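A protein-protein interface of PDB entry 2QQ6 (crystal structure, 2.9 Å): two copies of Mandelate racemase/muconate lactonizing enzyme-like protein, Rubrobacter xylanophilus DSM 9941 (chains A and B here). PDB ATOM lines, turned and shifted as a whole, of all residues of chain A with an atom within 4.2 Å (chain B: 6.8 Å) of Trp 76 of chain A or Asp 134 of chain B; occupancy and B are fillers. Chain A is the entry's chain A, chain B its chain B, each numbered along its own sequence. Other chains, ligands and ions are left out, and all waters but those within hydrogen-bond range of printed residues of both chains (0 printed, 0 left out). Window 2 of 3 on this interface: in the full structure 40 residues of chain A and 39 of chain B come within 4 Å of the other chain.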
ATOM      1  N   MET A  54      32.976  21.787  32.854  1.00  0.00           N
ATOM      2  CA  MET A  54      33.541  21.211  31.631  1.00  0.00           C
ATOM      3  C   MET A  54      34.705  20.248  31.904  1.00  0.00           C
ATOM      4  O   MET A  54      35.240  19.619  30.978  1.00  0.00           O
ATOM      5  CB  MET A  54      34.041  22.345  30.726  1.00  0.00           C
ATOM      6  CG  MET A  54      33.694  22.176  29.270  1.00  0.00           C
ATOM      7  SD  MET A  54      31.740  21.973  29.021  1.00  0.00           S
ATOM      8  CE  MET A  54      31.629  20.028  28.738  1.00  0.00           C
ATOM      9  N   GLN A  57      34.614  16.296  30.788  1.00  0.00           N
ATOM     10  CA  GLN A  57      34.902  16.124  29.373  1.00  0.00           C
ATOM     11  C   GLN A  57      36.372  16.270  29.062  1.00  0.00           C
ATOM     12  O   GLN A  57      36.862  15.728  28.069  1.00  0.00           O
ATOM     13  CB  GLN A  57      34.136  17.152  28.555  1.00  0.00           C
ATOM     14  CG  GLN A  57      32.652  17.129  28.783  1.00  0.00           C
ATOM     15  CD  GLN A  57      32.055  15.778  28.513  1.00  0.00           C
ATOM     16  OE1 GLN A  57      32.398  15.122  27.526  1.00  0.00           O
ATOM     17  NE2 GLN A  57      31.145  15.351  29.385  1.00  0.00           N
ATOM     18  N   LYS A  72      34.310  19.052  21.060  1.00  0.00           N
ATOM     19  CA  LYS A  72      33.783  18.151  22.070  1.00  0.00           C
ATOM     20  C   LYS A  72      32.943  18.896  23.121  1.00  0.00           C
ATOM     21  O   LYS A  72      31.766  18.589  23.328  1.00  0.00           O
ATOM     22  CB  LYS A  72      34.946  17.396  22.733  1.00  0.00           C
ATOM     23  CG  LYS A  72      34.534  16.314  23.734  1.00  0.00           C
ATOM     24  CD  LYS A  72      35.757  15.639  24.352  1.00  0.00           C
ATOM     25  CE  LYS A  72      35.379  14.779  25.553  1.00  0.00           C
ATOM     26  NZ  LYS A  72      34.508  13.661  25.145  1.00  0.00           N
ATOM     27  N   MET A  73      33.542  19.878  23.784  1.00  0.00           N
ATOM     28  CA  MET A  73      32.813  20.626  24.801  1.00  0.00           C
ATOM     29  C   MET A  73      31.692  21.409  24.130  1.00  0.00           C
ATOM     30  O   MET A  73      30.610  21.600  24.689  1.00  0.00           O
ATOM     31  CB  MET A  73      33.735  21.606  25.514  1.00  0.00           C
ATOM     32  CG  MET A  73      35.038  21.038  25.980  1.00  0.00           C
ATOM     33  SD  MET A  73      36.048  22.401  27.056  1.00  0.00           S
ATOM     34  CE  MET A  73      37.129  23.329  25.662  1.00  0.00           C
ATOM     35  N   ARG A  74      31.966  21.859  22.915  1.00  0.00           N
ATOM     36  CA  ARG A  74      31.000  22.643  22.188  1.00  0.00           C
ATOM     37  C   ARG A  74      29.736  21.863  21.863  1.00  0.00           C
ATOM     38  O   ARG A  74      28.624  22.344  22.112  1.00  0.00           O
ATOM     39  CB  ARG A  74      31.621  23.192  20.911  1.00  0.00           C
ATOM     40  CG  ARG A  74      30.840  24.359  20.386  1.00  0.00           C
ATOM     41  CD  ARG A  74      31.272  24.788  19.020  1.00  0.00           C
ATOM     42  NE  ARG A  74      30.089  25.005  18.206  1.00  0.00           N
ATOM     43  CZ  ARG A  74      29.501  24.064  17.482  1.00  0.00           C
ATOM     44  NH1 ARG A  74      29.996  22.834  17.455  1.00  0.00           N
ATOM     45  NH2 ARG A  74      28.398  24.352  16.807  1.00  0.00           N
ATOM     46  N   ARG A  75      29.906  20.664  21.312  1.00  0.00           N
ATOM     47  CA  ARG A  75      28.756  19.835  20.965  1.00  0.00           C
ATOM     48  C   ARG A  75      28.068  19.261  22.188  1.00  0.00           C
ATOM     49  O   ARG A  75      26.914  18.851  22.115  1.00  0.00           O
ATOM     50  CB  ARG A  75      29.164  18.694  20.033  1.00  0.00           C
ATOM     51  CG  ARG A  75      29.825  19.179  18.759  1.00  0.00           C
ATOM     52  CD  ARG A  75      29.977  18.089  17.700  1.00  0.00           C
ATOM     53  NE  ARG A  75      30.776  18.597  16.589  1.00  0.00           N
ATOM     54  CZ  ARG A  75      30.935  17.989  15.422  1.00  0.00           C
ATOM     55  NH1 ARG A  75      30.346  16.827  15.176  1.00  0.00           N
ATOM     56  NH2 ARG A  75      31.710  18.550  14.504  1.00  0.00           N
ATOM     57  N   TRP A  76      28.782  19.237  23.310  1.00  0.00           N
ATOM     58  CA  TRP A  76      28.240  18.719  24.563  1.00  0.00           C
ATOM     59  C   TRP A  76      27.236  19.714  25.176  1.00  0.00           C
ATOM     60  O   TRP A  76      26.384  19.345  25.987  1.00  0.00           O
ATOM     61  CB  TRP A  76      29.403  18.411  25.527  1.00  0.00           C
ATOM     62  CG  TRP A  76      28.987  17.959  26.907  1.00  0.00           C
ATOM     63  CD1 TRP A  76      28.910  18.735  28.030  1.00  0.00           C
ATOM     64  CD2 TRP A  76      28.503  16.659  27.289  1.00  0.00           C
ATOM     65  NE1 TRP A  76      28.403  18.005  29.082  1.00  0.00           N
ATOM     66  CE2 TRP A  76      28.144  16.729  28.655  1.00  0.00           C
ATOM     67  CE3 TRP A  76      28.334  15.443  26.609  1.00  0.00           C
ATOM     68  CZ2 TRP A  76      27.624  15.635  29.349  1.00  0.00           C
ATOM     69  CZ3 TRP A  76      27.815  14.353  27.306  1.00  0.00           C
ATOM     70  CH2 TRP A  76      27.467  14.462  28.660  1.00  0.00           C
ATOM     71  N   ASN A  77      27.314  20.968  24.739  1.00  0.00           N
ATOM     72  CA  ASN A  77      26.444  22.036  25.230  1.00  0.00           C
ATOM     73  C   ASN A  77      25.346  22.415  24.236  1.00  0.00           C
ATOM     74  O   ASN A  77      24.682  23.440  24.387  1.00  0.00           O
ATOM     75  CB  ASN A  77      27.294  23.271  25.542  1.00  0.00           C
ATOM     76  CG  ASN A  77      28.210  23.077  26.749  1.00  0.00           C
ATOM     77  OD1 ASN A  77      27.795  23.285  27.889  1.00  0.00           O
ATOM     78  ND2 ASN A  77      29.459  22.676  26.499  1.00  0.00           N
ATOM     79  N   ILE A  78      25.169  21.589  23.213  1.00  0.00           N
ATOM     80  CA  ILE A  78      24.162  21.834  22.190  1.00  0.00           C
ATOM     81  C   ILE A  78      22.785  22.089  22.782  1.00  0.00           C
ATOM     82  O   ILE A  78      22.061  22.959  22.313  1.00  0.00           O
ATOM     83  CB  ILE A  78      24.059  20.649  21.230  1.00  0.00           C
ATOM     84  CG1 ILE A  78      22.782  20.770  20.388  1.00  0.00           C
ATOM     85  CG2 ILE A  78      24.092  19.354  22.022  1.00  0.00           C
ATOM     86  CD1 ILE A  78      22.517  19.598  19.481  1.00  0.00           C
ATOM     87  N   GLY B 131      13.538   8.802  29.989  1.00  0.00           N
ATOM     88  CA  GLY B 131      14.571   8.324  30.898  1.00  0.00           C
ATOM     89  C   GLY B 131      15.958   8.040  30.331  1.00  0.00           C
ATOM     90  O   GLY B 131      16.922   7.899  31.098  1.00  0.00           O
ATOM     91  N   THR B 132      16.059   7.954  29.002  1.00  0.00           N
ATOM     92  CA  THR B 132      17.310   7.668  28.282  1.00  0.00           C
ATOM     93  C   THR B 132      18.294   8.827  28.312  1.00  0.00           C
ATOM     94  O   THR B 132      19.459   8.689  27.914  1.00  0.00           O
ATOM     95  CB  THR B 132      17.040   7.392  26.789  1.00  0.00           C
ATOM     96  OG1 THR B 132      15.711   6.865  26.614  1.00  0.00           O
ATOM     97  CG2 THR B 132      18.098   6.411  26.231  1.00  0.00           C
ATOM     98  N   VAL B 133      17.783   9.965  28.764  1.00  0.00           N
ATOM     99  CA  VAL B 133      18.492  11.230  28.875  1.00  0.00           C
ATOM    100  C   VAL B 133      19.979  11.334  29.236  1.00  0.00           C
ATOM    101  O   VAL B 133      20.409  10.965  30.334  1.00  0.00           O
ATOM    102  CB  VAL B 133      17.713  12.175  29.854  1.00  0.00           C
ATOM    103  CG1 VAL B 133      18.566  13.424  30.194  1.00  0.00           C
ATOM    104  CG2 VAL B 133      16.371  12.603  29.228  1.00  0.00           C
ATOM    105  N   ASP B 134      20.759  11.859  28.299  1.00  0.00           N
ATOM    106  CA  ASP B 134      22.161  12.107  28.561  1.00  0.00           C
ATOM    107  C   ASP B 134      22.154  13.629  28.626  1.00  0.00           C
ATOM    108  O   ASP B 134      21.297  14.270  28.018  1.00  0.00           O
ATOM    109  CB  ASP B 134      23.037  11.652  27.407  1.00  0.00           C
ATOM    110  CG  ASP B 134      24.484  12.069  27.582  1.00  0.00           C
ATOM    111  OD1 ASP B 134      24.756  13.279  27.696  1.00  0.00           O
ATOM    112  OD2 ASP B 134      25.362  11.185  27.606  1.00  0.00           O
ATOM    113  N   ALA B 135      23.071  14.224  29.372  1.00  0.00           N
ATOM    114  CA  ALA B 135      23.096  15.676  29.447  1.00  0.00           C
ATOM    115  C   ALA B 135      23.069  16.266  28.041  1.00  0.00           C
ATOM    116  O   ALA B 135      22.482  17.328  27.812  1.00  0.00           O
ATOM    117  CB  ALA B 135      24.332  16.127  30.162  1.00  0.00           C
ATOM    118  N   ALA B 136      23.712  15.578  27.100  1.00  0.00           N
ATOM    119  CA  ALA B 136      23.766  16.039  25.724  1.00  0.00           C
ATOM    120  C   ALA B 136      22.810  15.263  24.829  1.00  0.00           C
ATOM    121  O   ALA B 136      23.061  15.104  23.641  1.00  0.00           O
ATOM    122  CB  ALA B 136      25.177  15.928  25.195  1.00  0.00           C
ATOM    123  N   ALA B 137      21.718  14.770  25.397  1.00  0.00           N
ATOM    124  CA  ALA B 137      20.707  14.037  24.626  1.00  0.00           C
ATOM    125  C   ALA B 137      21.152  12.719  24.004  1.00  0.00           C
ATOM    126  O   ALA B 137      20.543  12.247  23.038  1.00  0.00           O
ATOM    127  CB  ALA B 137      20.125  14.941  23.535  1.00  0.00           C
ATOM    128  N   HIS B 138      22.217  12.128  24.537  1.00  0.00           N
ATOM    129  CA  HIS B 138      22.676  10.843  24.026  1.00  0.00           C
ATOM    130  C   HIS B 138      21.948   9.720  24.764  1.00  0.00           C
ATOM    131  O   HIS B 138      21.438   9.923  25.870  1.00  0.00           O
ATOM    132  CB  HIS B 138      24.186  10.745  24.171  1.00  0.00           C
ATOM    133  CG  HIS B 138      24.921  11.566  23.160  1.00  0.00           C
ATOM    134  ND1 HIS B 138      24.837  11.319  21.806  1.00  0.00           N
ATOM    135  CD2 HIS B 138      25.717  12.652  23.295  1.00  0.00           C
ATOM    136  CE1 HIS B 138      25.550  12.218  21.151  1.00  0.00           C
ATOM    137  NE2 HIS B 138      26.094  13.039  22.031  1.00  0.00           N
ATOM    138  N   HIS B 139      21.873   8.542  24.157  1.00  0.00           N
ATOM    139  CA  HIS B 139      21.136   7.460  24.787  1.00  0.00           C
ATOM    140  C   HIS B 139      21.965   6.498  25.594  1.00  0.00           C
ATOM    141  O   HIS B 139      22.838   5.803  25.077  1.00  0.00           O
ATOM    142  CB  HIS B 139      20.295   6.741  23.740  1.00  0.00           C
ATOM    143  CG  HIS B 139      19.394   7.670  22.992  1.00  0.00           C
ATOM    144  ND1 HIS B 139      19.845   8.468  21.961  1.00  0.00           N
ATOM    145  CD2 HIS B 139      18.104   8.020  23.202  1.00  0.00           C
ATOM    146  CE1 HIS B 139      18.873   9.272  21.572  1.00  0.00           C
ATOM    147  NE2 HIS B 139      17.806   9.022  22.309  1.00  0.00           N
ATOM    148  N   ILE B 140      21.647   6.490  26.884  1.00  0.00           N
ATOM    149  CA  ILE B 140      22.299   5.691  27.913  1.00  0.00           C
ATOM    150  C   ILE B 140      22.075   4.179  27.856  1.00  0.00           C
ATOM    151  O   ILE B 140      21.062   3.703  27.337  1.00  0.00           O
ATOM    152  CB  ILE B 140      21.841   6.190  29.298  1.00  0.00           C
ATOM    153  CG1 ILE B 140      20.327   5.969  29.443  1.00  0.00           C
ATOM    154  CG2 ILE B 140      22.189   7.670  29.455  1.00  0.00           C
ATOM    155  CD1 ILE B 140      19.716   6.563  30.691  1.00  0.00           C
ATOM    156  N   THR B 176      26.576   7.298  19.491  1.00  0.00           N
ATOM    157  CA  THR B 176      27.515   6.579  20.334  1.00  0.00           C
ATOM    158  C   THR B 176      27.237   5.086  20.235  1.00  0.00           C
ATOM    159  O   THR B 176      27.822   4.286  20.962  1.00  0.00           O
ATOM    160  CB  THR B 176      27.355   6.994  21.786  1.00  0.00           C
ATOM    161  OG1 THR B 176      26.036   6.653  22.223  1.00  0.00           O
ATOM    162  CG2 THR B 176      27.540   8.483  21.933  1.00  0.00           C
ATOM    163  N   ARG B 220      22.047  15.915  14.483  1.00  0.00           N
ATOM    164  CA  ARG B 220      23.397  15.362  14.480  1.00  0.00           C
ATOM    165  C   ARG B 220      23.914  14.989  13.098  1.00  0.00           C
ATOM    166  O   ARG B 220      25.020  14.454  13.003  1.00  0.00           O
ATOM    167  CB  ARG B 220      23.465  14.073  15.317  1.00  0.00           C
ATOM    168  CG  ARG B 220      22.586  13.999  16.542  1.00  0.00           C
ATOM    169  CD  ARG B 220      23.276  14.514  17.777  1.00  0.00           C
ATOM    170  NE  ARG B 220      22.533  14.127  18.969  1.00  0.00           N
ATOM    171  CZ  ARG B 220      22.861  14.488  20.201  1.00  0.00           C
ATOM    172  NH1 ARG B 220      23.925  15.254  20.413  1.00  0.00           N
ATOM    173  NH2 ARG B 220      22.123  14.082  21.219  1.00  0.00           N
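No position is printed for both chains.
Gly 131 of chain B touches none of the printed residues of chain A.
Asp 134 of chain B touches one residue of chain A.
Of the printed residues of chain A, Ala 135 of chain B touches Trp 76.
Printed residues of chain A within 4 Å of Ala 136 of chain B: Trp 76 (3.5 Å).
His 138 of chain B touches none of the printed residues of chain A.
The nearest residue of chain B that does not touch Trp 76 of chain A is His 138 of chain B (4.8 Å).
The nearest printed residue of chain A that does not touch Asp 134 of chain B is Gln 57 of chain A (6.9 Å).
Printed residues of chain B that touch a printed residue of chain A: Asp 134, Ala 135 and Ala 136.
Hydrophobic or aromatic side chains of chain B within 4 Å of the printed part of chain A: Ala 135 and Ala 136.
Of the 9 printed residues of chain A, 1 touches a printed residue of chain B.
Printed residues of chain A that touch a printed residue of chain B: Trp 76.
Hydrophobic or aromatic side chains of chain A within 4 Å of the printed part of chain B: Trp 76.
Among the printed residues, merely in contact across the chains: Trp 76 of chain A with Asp 134 of chain B (3.1 Å), Trp 76 of chain A with Ala 135 of chain B (3.4 Å) and Trp 76 of chain A with Ala 136 of chain B (3.5 Å).
The backbone NH (N) of Ala 136 of chain B is in hydrogen-bond range of the side-chain carboxylate (OD1) of Asp 134 of chain B, at 2.6 Å.
The guanidinium group of Arg 220 of chain B lies within hydrogen-bond range of the backbone carbonyl oxygen of Ala 136 of chain B, 2.8 Å away.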
